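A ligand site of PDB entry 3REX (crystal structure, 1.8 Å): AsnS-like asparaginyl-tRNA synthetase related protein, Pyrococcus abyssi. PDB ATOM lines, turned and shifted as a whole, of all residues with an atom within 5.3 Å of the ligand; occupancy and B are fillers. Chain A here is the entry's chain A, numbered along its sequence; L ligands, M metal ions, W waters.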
ATOM      1  N   ASP A  47     -15.414   7.339  25.885  1.00  0.00           N
ATOM      2  CA  ASP A  47     -16.382   8.436  26.052  1.00  0.00           C
ATOM      3  C   ASP A  47     -16.391   8.907  27.495  1.00  0.00           C
ATOM      4  O   ASP A  47     -16.610   8.110  28.401  1.00  0.00           O
ATOM      5  CB  ASP A  47     -17.757   7.877  25.669  1.00  0.00           C
ATOM      6  CG  ASP A  47     -18.827   8.946  25.518  1.00  0.00           C
ATOM      7  OD1 ASP A  47     -18.652  10.084  26.006  1.00  0.00           O
ATOM      8  OD2 ASP A  47     -19.859   8.624  24.896  1.00  0.00           O
ATOM      9  N   LEU A  49     -18.592  10.821  28.931  1.00  0.00           N
ATOM     10  CA  LEU A  49     -19.999  10.890  29.373  1.00  0.00           C
ATOM     11  C   LEU A  49     -20.208  12.132  30.217  1.00  0.00           C
ATOM     12  O   LEU A  49     -21.109  12.180  31.049  1.00  0.00           O
ATOM     13  CB  LEU A  49     -20.396   9.640  30.178  1.00  0.00           C
ATOM     14  CG  LEU A  49     -20.317   8.310  29.402  1.00  0.00           C
ATOM     15  CD1 LEU A  49     -20.759   7.111  30.272  1.00  0.00           C
ATOM     16  CD2 LEU A  49     -21.165   8.392  28.161  1.00  0.00           C
ATOM     17  N   SER A  75     -18.570   4.279  25.673  1.00  0.00           N
ATOM     18  CA  SER A  75     -19.190   4.213  24.341  1.00  0.00           C
ATOM     19  C   SER A  75     -18.074   4.289  23.312  1.00  0.00           C
ATOM     20  O   SER A  75     -16.960   4.689  23.627  1.00  0.00           O
ATOM     21  CB  SER A  75     -20.263   5.309  24.106  1.00  0.00           C
ATOM     22  OG  SER A  75     -19.811   6.356  23.232  1.00  0.00           O
ATOM     23  N   ASN A  97     -21.721  -1.635  26.074  1.00  0.00           N
ATOM     24  CA  ASN A  97     -21.119  -0.599  26.922  1.00  0.00           C
ATOM     25  C   ASN A  97     -21.158  -1.050  28.375  1.00  0.00           C
ATOM     26  O   ASN A  97     -22.031  -1.826  28.757  1.00  0.00           O
ATOM     27  CB  ASN A  97     -21.862   0.730  26.799  1.00  0.00           C
ATOM     28  CG  ASN A  97     -21.798   1.324  25.389  1.00  0.00           C
ATOM     29  OD1 ASN A  97     -20.979   0.933  24.555  1.00  0.00           O
ATOM     30  ND2 ASN A  97     -22.631   2.326  25.149  1.00  0.00           N
ATOM     31  N   ARG A  99     -21.365   0.823  32.019  1.00  0.00           N
ATOM     32  CA  ARG A  99     -21.505   2.086  32.739  1.00  0.00           C
ATOM     33  C   ARG A  99     -21.991   1.795  34.135  1.00  0.00           C
ATOM     34  O   ARG A  99     -23.155   1.458  34.343  1.00  0.00           O
ATOM     35  CB  ARG A  99     -22.491   2.992  32.013  1.00  0.00           C
ATOM     36  CG  ARG A  99     -22.053   3.285  30.583  1.00  0.00           C
ATOM     37  CD  ARG A  99     -22.964   4.275  29.908  1.00  0.00           C
ATOM     38  NE  ARG A  99     -22.642   4.398  28.490  1.00  0.00           N
ATOM     39  CZ  ARG A  99     -23.257   5.243  27.665  1.00  0.00           C
ATOM     40  NH1 ARG A  99     -24.219   6.041  28.132  1.00  0.00           N
ATOM     41  NH2 ARG A  99     -22.929   5.278  26.390  1.00  0.00           N
ATOM     42  N   GLU A 101     -23.310   2.983  36.698  1.00  0.00           N
ATOM     43  CA  GLU A 101     -24.118   4.052  37.263  1.00  0.00           C
ATOM     44  C   GLU A 101     -24.688   3.662  38.632  1.00  0.00           C
ATOM     45  O   GLU A 101     -24.739   2.485  39.000  1.00  0.00           O
ATOM     46  CB  GLU A 101     -25.207   4.477  36.263  1.00  0.00           C
ATOM     47  CG  GLU A 101     -24.602   4.878  34.913  1.00  0.00           C
ATOM     48  CD  GLU A 101     -25.575   5.541  33.949  1.00  0.00           C
ATOM     49  OE1 GLU A 101     -25.934   6.718  34.178  1.00  0.00           O
ATOM     50  OE2 GLU A 101     -25.951   4.883  32.951  1.00  0.00           O
ATOM     51  N   ARG A 109     -35.090   2.036  33.145  1.00  0.00           N
ATOM     52  CA  ARG A 109     -34.595   2.338  31.812  1.00  0.00           C
ATOM     53  C   ARG A 109     -33.081   2.094  31.691  1.00  0.00           C
ATOM     54  O   ARG A 109     -32.522   2.029  30.586  1.00  0.00           O
ATOM     55  CB  ARG A 109     -34.918   3.819  31.541  1.00  0.00           C
ATOM     56  CG  ARG A 109     -34.703   4.321  30.161  1.00  0.00           C
ATOM     57  CD  ARG A 109     -35.456   5.636  29.943  1.00  0.00           C
ATOM     58  NE  ARG A 109     -35.012   6.718  30.815  1.00  0.00           N
ATOM     59  CZ  ARG A 109     -35.713   7.198  31.845  1.00  0.00           C
ATOM     60  NH1 ARG A 109     -36.897   6.672  32.144  1.00  0.00           N
ATOM     61  NH2 ARG A 109     -35.233   8.194  32.577  1.00  0.00           N
ATOM     62  N   HIS A 110     -32.406   1.938  32.834  1.00  0.00           N
ATOM     63  CA  HIS A 110     -30.950   1.775  32.830  1.00  0.00           C
ATOM     64  C   HIS A 110     -30.469   0.385  33.227  1.00  0.00           C
ATOM     65  O   HIS A 110     -31.031  -0.251  34.132  1.00  0.00           O
ATOM     66  CB  HIS A 110     -30.288   2.777  33.791  1.00  0.00           C
ATOM     67  CG  HIS A 110     -30.389   4.203  33.362  1.00  0.00           C
ATOM     68  ND1 HIS A 110     -31.533   4.947  33.510  1.00  0.00           N
ATOM     69  CD2 HIS A 110     -29.460   5.034  32.821  1.00  0.00           C
ATOM     70  CE1 HIS A 110     -31.320   6.179  33.069  1.00  0.00           C
ATOM     71  NE2 HIS A 110     -30.071   6.250  32.646  1.00  0.00           N
ATOM     72  N   SER A 111     -29.395  -0.060  32.578  1.00  0.00           N
ATOM     73  CA  SER A 111     -28.693  -1.286  32.920  1.00  0.00           C
ATOM     74  C   SER A 111     -27.191  -0.986  32.941  1.00  0.00           C
ATOM     75  O   SER A 111     -26.714  -0.164  32.160  1.00  0.00           O
ATOM     76  CB  SER A 111     -29.004  -2.342  31.856  1.00  0.00           C
ATOM     77  OG  SER A 111     -28.441  -3.582  32.210  1.00  0.00           O
ATOM     78  N   TYR A 112     -26.425  -1.627  33.807  1.00  0.00           N
ATOM     79  CA  TYR A 112     -25.006  -1.277  33.833  1.00  0.00           C
ATOM     80  C   TYR A 112     -24.173  -1.944  32.736  1.00  0.00           C
ATOM     81  O   TYR A 112     -23.033  -1.548  32.499  1.00  0.00           O
ATOM     82  CB  TYR A 112     -24.376  -1.379  35.225  1.00  0.00           C
ATOM     83  CG  TYR A 112     -24.119  -2.777  35.777  1.00  0.00           C
ATOM     84  CD1 TYR A 112     -23.021  -3.522  35.367  1.00  0.00           C
ATOM     85  CD2 TYR A 112     -24.938  -3.308  36.771  1.00  0.00           C
ATOM     86  CE1 TYR A 112     -22.760  -4.783  35.917  1.00  0.00           C
ATOM     87  CE2 TYR A 112     -24.693  -4.575  37.316  1.00  0.00           C
ATOM     88  CZ  TYR A 112     -23.607  -5.296  36.881  1.00  0.00           C
ATOM     89  OH  TYR A 112     -23.368  -6.540  37.419  1.00  0.00           O
ATOM     90  N   PHE A 114     -25.144  -2.882  28.618  1.00  0.00           N
ATOM     91  CA  PHE A 114     -26.199  -2.850  27.609  1.00  0.00           C
ATOM     92  C   PHE A 114     -25.541  -2.745  26.238  1.00  0.00           C
ATOM     93  O   PHE A 114     -24.349  -2.495  26.143  1.00  0.00           O
ATOM     94  CB  PHE A 114     -27.143  -1.661  27.859  1.00  0.00           C
ATOM     95  CG  PHE A 114     -26.497  -0.331  27.619  1.00  0.00           C
ATOM     96  CD1 PHE A 114     -26.596   0.299  26.386  1.00  0.00           C
ATOM     97  CD2 PHE A 114     -25.761   0.279  28.641  1.00  0.00           C
ATOM     98  CE1 PHE A 114     -25.973   1.521  26.158  1.00  0.00           C
ATOM     99  CE2 PHE A 114     -25.142   1.493  28.436  1.00  0.00           C
ATOM    100  CZ  PHE A 114     -25.250   2.127  27.207  1.00  0.00           C
ATOM    101  N   GLN A 116     -25.773  -0.825  22.374  1.00  0.00           N
ATOM    102  CA  GLN A 116     -26.375   0.172  21.500  1.00  0.00           C
ATOM    103  C   GLN A 116     -25.940  -0.074  20.075  1.00  0.00           C
ATOM    104  O   GLN A 116     -24.796  -0.421  19.826  1.00  0.00           O
ATOM    105  CB  GLN A 116     -26.055   1.626  21.919  1.00  0.00           C
ATOM    106  CG  GLN A 116     -24.575   1.984  22.050  1.00  0.00           C
ATOM    107  CD  GLN A 116     -24.359   3.488  22.212  1.00  0.00           C
ATOM    108  OE1 GLN A 116     -24.591   4.248  21.280  1.00  0.00           O
ATOM    109  NE2 GLN A 116     -23.924   3.915  23.386  1.00  0.00           N
ATOM    110  N   GLU A 215     -35.769   8.241  26.875  1.00  0.00           N
ATOM    111  CA  GLU A 215     -34.866   8.287  25.725  1.00  0.00           C
ATOM    112  C   GLU A 215     -34.542   6.919  25.150  1.00  0.00           C
ATOM    113  O   GLU A 215     -34.279   5.976  25.884  1.00  0.00           O
ATOM    114  CB  GLU A 215     -33.575   9.025  26.133  1.00  0.00           C
ATOM    115  CG  GLU A 215     -32.433   8.956  25.127  1.00  0.00           C
ATOM    116  CD  GLU A 215     -31.103   9.275  25.803  1.00  0.00           C
ATOM    117  OE1 GLU A 215     -31.094   9.957  26.864  1.00  0.00           O
ATOM    118  OE2 GLU A 215     -30.060   8.818  25.306  1.00  0.00           O
ATOM    119  N   VAL A 216     -34.559   6.804  23.819  1.00  0.00           N
ATOM    120  CA  VAL A 216     -34.185   5.549  23.157  1.00  0.00           C
ATOM    121  C   VAL A 216     -33.008   5.713  22.164  1.00  0.00           C
ATOM    122  O   VAL A 216     -32.333   4.746  21.790  1.00  0.00           O
ATOM    123  CB  VAL A 216     -35.419   4.922  22.464  1.00  0.00           C
ATOM    124  CG1 VAL A 216     -35.838   5.748  21.255  1.00  0.00           C
ATOM    125  CG2 VAL A 216     -35.150   3.486  22.035  1.00  0.00           C
ATOM    126  N   SER A 217     -32.724   6.956  21.772  1.00  0.00           N
ATOM    127  CA  SER A 217     -31.623   7.236  20.851  1.00  0.00           C
ATOM    128  C   SER A 217     -31.042   8.622  21.106  1.00  0.00           C
ATOM    129  O   SER A 217     -31.747   9.519  21.552  1.00  0.00           O
ATOM    130  CB  SER A 217     -32.105   7.103  19.393  1.00  0.00           C
ATOM    131  OG  SER A 217     -31.032   7.254  18.464  1.00  0.00           O
ATOM    132  N   SER A 218     -29.739   8.770  20.850  1.00  0.00           N
ATOM    133  CA  SER A 218     -29.070  10.051  21.105  1.00  0.00           C
ATOM    134  C   SER A 218     -27.906  10.167  20.125  1.00  0.00           C
ATOM    135  O   SER A 218     -27.224   9.193  19.856  1.00  0.00           O
ATOM    136  CB  SER A 218     -28.575  10.083  22.550  1.00  0.00           C
ATOM    137  OG  SER A 218     -27.965  11.303  22.857  1.00  0.00           O
ATOM    138  N   GLY A 262     -26.668   6.621  18.484  1.00  0.00           N
ATOM    139  CA  GLY A 262     -26.761   5.280  19.031  1.00  0.00           C
ATOM    140  C   GLY A 262     -28.198   5.005  19.407  1.00  0.00           C
ATOM    141  O   GLY A 262     -28.914   5.915  19.815  1.00  0.00           O
ATOM    142  N   ILE A 263     -28.619   3.751  19.248  1.00  0.00           N
ATOM    143  CA  ILE A 263     -29.991   3.343  19.545  1.00  0.00           C
ATOM    144  C   ILE A 263     -29.901   2.215  20.573  1.00  0.00           C
ATOM    145  O   ILE A 263     -29.249   1.210  20.313  1.00  0.00           O
ATOM    146  CB  ILE A 263     -30.696   2.781  18.287  1.00  0.00           C
ATOM    147  CG1 ILE A 263     -30.760   3.843  17.189  1.00  0.00           C
ATOM    148  CG2 ILE A 263     -32.098   2.282  18.643  1.00  0.00           C
ATOM    149  CD1 ILE A 263     -31.150   3.302  15.816  1.00  0.00           C
ATOM    150  N   GLY A 264     -30.534   2.394  21.727  1.00  0.00           N
ATOM    151  CA  GLY A 264     -30.466   1.392  22.784  1.00  0.00           C
ATOM    152  C   GLY A 264     -31.282   0.166  22.430  1.00  0.00           C
ATOM    153  O   GLY A 264     -32.509   0.244  22.347  1.00  0.00           O
ATOM    154  N   GLU A 266     -31.913  -2.809  24.135  1.00  0.00           N
ATOM    155  CA  GLU A 266     -32.760  -3.260  25.233  1.00  0.00           C
ATOM    156  C   GLU A 266     -33.899  -2.277  25.503  1.00  0.00           C
ATOM    157  O   GLU A 266     -35.027  -2.678  25.745  1.00  0.00           O
ATOM    158  CB  GLU A 266     -31.928  -3.461  26.514  1.00  0.00           C
ATOM    159  CG  GLU A 266     -30.877  -4.602  26.441  1.00  0.00           C
ATOM    160  CD  GLU A 266     -29.501  -4.144  25.951  1.00  0.00           C
ATOM    161  OE1 GLU A 266     -29.388  -3.036  25.359  1.00  0.00           O
ATOM    162  OE2 GLU A 266     -28.514  -4.894  26.169  1.00  0.00           O
ATOM    163  N   ARG A 267     -33.612  -0.981  25.448  1.00  0.00           N
ATOM    164  CA  ARG A 267     -34.673   0.025  25.668  1.00  0.00           C
ATOM    165  C   ARG A 267     -35.771  -0.124  24.608  1.00  0.00           C
ATOM    166  O   ARG A 267     -36.953  -0.013  24.920  1.00  0.00           O
ATOM    167  CB  ARG A 267     -34.115   1.442  25.653  1.00  0.00           C
ATOM    168  CG  ARG A 267     -33.290   1.772  26.911  1.00  0.00           C
ATOM    169  CD  ARG A 267     -33.086   3.282  27.089  1.00  0.00           C
ATOM    170  NE  ARG A 267     -32.312   3.563  28.299  1.00  0.00           N
ATOM    171  CZ  ARG A 267     -31.875   4.762  28.674  1.00  0.00           C
ATOM    172  NH1 ARG A 267     -32.133   5.829  27.925  1.00  0.00           N
ATOM    173  NH2 ARG A 267     -31.167   4.879  29.791  1.00  0.00           N
ATOM    174  N   ILE A 278     -36.473  -2.668  32.381  1.00  0.00           N
ATOM    175  CA  ILE A 278     -35.543  -3.203  31.395  1.00  0.00           C
ATOM    176  C   ILE A 278     -34.931  -4.553  31.796  1.00  0.00           C
ATOM    177  O   ILE A 278     -34.601  -5.370  30.945  1.00  0.00           O
ATOM    178  CB  ILE A 278     -34.431  -2.166  31.075  1.00  0.00           C
ATOM    179  CG1 ILE A 278     -33.754  -2.457  29.744  1.00  0.00           C
ATOM    180  CG2 ILE A 278     -33.413  -2.080  32.216  1.00  0.00           C
ATOM    181  CD1 ILE A 278     -32.730  -1.414  29.373  1.00  0.00           C
HETATM  182  P1  LIG L   1     -25.431   7.313  24.746  1.00  0.00           P
HETATM  183  O1  LIG L   1     -25.849   8.529  23.976  1.00  0.00           O
HETATM  184  O2  LIG L   1     -24.113   6.655  24.394  1.00  0.00           O
HETATM  185  O3  LIG L   1     -25.464   7.616  26.251  1.00  0.00           O
HETATM  186  O4  LIG L   1     -26.579   6.222  24.709  1.00  0.00           O
HETATM  187  C1  LIG L   1     -27.101   5.758  23.471  1.00  0.00           C
HETATM  188  C2  LIG L   1     -28.367   4.991  23.710  1.00  0.00           C
HETATM  189  O5  LIG L   1     -28.064   3.816  24.497  1.00  0.00           O
HETATM  190  C3  LIG L   1     -29.419   5.736  24.523  1.00  0.00           C
HETATM  191  O6  LIG L   1     -30.214   6.605  23.739  1.00  0.00           O
HETATM  192  C4  LIG L   1     -30.198   4.608  25.188  1.00  0.00           C
HETATM  193  O7  LIG L   1     -31.153   4.072  24.291  1.00  0.00           O
HETATM  194  C5  LIG L   1     -29.117   3.561  25.400  1.00  0.00           C
HETATM  195  N1  LIG L   1     -28.561   3.609  26.757  1.00  0.00           N
HETATM  196  C6  LIG L   1     -27.733   4.564  27.238  1.00  0.00           C
HETATM  197  N2  LIG L   1     -27.412   4.296  28.537  1.00  0.00           N
HETATM  198  C7  LIG L   1     -28.057   3.163  28.878  1.00  0.00           C
HETATM  199  C8  LIG L   1     -28.130   2.325  30.079  1.00  0.00           C
HETATM  200  N3  LIG L   1     -27.459   2.668  31.206  1.00  0.00           N
HETATM  201  N4  LIG L   1     -28.914   1.224  30.013  1.00  0.00           N
HETATM  202  C9  LIG L   1     -29.587   0.862  28.897  1.00  0.00           C
HETATM  203  N5  LIG L   1     -29.556   1.581  27.758  1.00  0.00           N
HETATM  204  C10 LIG L   1     -28.813   2.709  27.702  1.00  0.00           C
HETATM  205 MG    MG M   1     -25.536  11.458  26.762  1.00  0.00          MG
HETATM  206  O   HOH W   1     -26.766  10.465  25.220  1.00  0.00           O
HETATM  207  O   HOH W   2     -24.067   9.863  26.801  1.00  0.00           O
HETATM  208  O   HOH W   3     -26.135   5.941  30.561  1.00  0.00           O
HETATM  209  O   HOH W   4     -27.818   8.157  27.293  1.00  0.00           O
HETATM  210  O   HOH W   5     -30.570  -0.127  25.677  1.00  0.00           O
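The side-chain amide nitrogen (NE2) of Gln 116 sits close to the guanidinium group (NH2) of Arg 99 (3.4 Å). The backbone NH (N) of Arg 99 sits at hydrogen-bond distance from the backbone carbonyl oxygen (O) of Tyr 112 (2.9 Å). The backbone carbonyl oxygen (O) of Glu 215 sits at hydrogen-bond distance from the guanidinium group (NH1) of Arg 267, 3.0 Å away. The backbone carbonyl oxygen (O) of Val 216 lies within hydrogen-bond range of the backbone NH (N) of Gly 264 (3.0 Å). ND2 of Asn 97 lies close to NE2 of Gln 116. O of Gly 262 sits at hydrogen-bond distance from OG of Ser 217 (2.8 Å). NE of Arg 267 sits at hydrogen-bond distance from O of Arg 109 (2.8 Å). O of Ser 218 is in hydrogen-bond range of N of Gly 262.
Residues that only touch the ligand: Phe 114, Ser 218, His 110, Arg 109 and Ile 278. Of the 22 residues printed, 14 come within 4 Å of the ligand.
Water W1 bridges O1 of the ligand and OG of Ser 218. Water W4 bridges O3 of the ligand (2.6 Å) and OE2 of Glu 215 (3.1 Å). Water W5 lies within hydrogen-bond range of a nitrogen (N5) of the ligand, the side-chain carboxylate (OE1) of Glu 266 and the backbone NH (N) of Arg 267. Water W3 lies within hydrogen-bond range of the side-chain carboxylate (OE2) of Glu 101 (2.6 Å), a nitrogen (N2) of the ligand (2.9 Å) and the guanidinium group (NH1) of Arg 99 (3.1 Å).
NH2 of Arg 99 lies within salt-bridge range of O2 of the ligand (2.7 Å). The side-chain carboxylate of Glu 215 is in hydrogen-bond range of an oxygen (O6) of the ligand (2.7 Å). The backbone carbonyl oxygen of Val 216 lies within hydrogen-bond range of an oxygen (O7) of the ligand. N of Ser 111 lies within hydrogen-bond range of N4 of the ligand (2.9 Å). The backbone carbonyl oxygen (O) of Ser 111 sits at hydrogen-bond distance from a nitrogen (N3) of the ligand, 3.1 Å away. An oxygen (O2) of the ligand lies within hydrogen-bond range of the side-chain amide nitrogen (NE2) of Gln 116 (2.9 Å). O7 of the ligand is in hydrogen-bond range of N of Gly 264 (3.1 Å). OE2 of Glu 101 sits at hydrogen-bond distance from N3 of the ligand, 3.2 Å away. N of Ser 217 lies within hydrogen-bond range of O6 of the ligand. A nitrogen (N5) of the ligand is in hydrogen-bond range of the guanidinium group (NE) of Arg 267 (3.4 Å).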
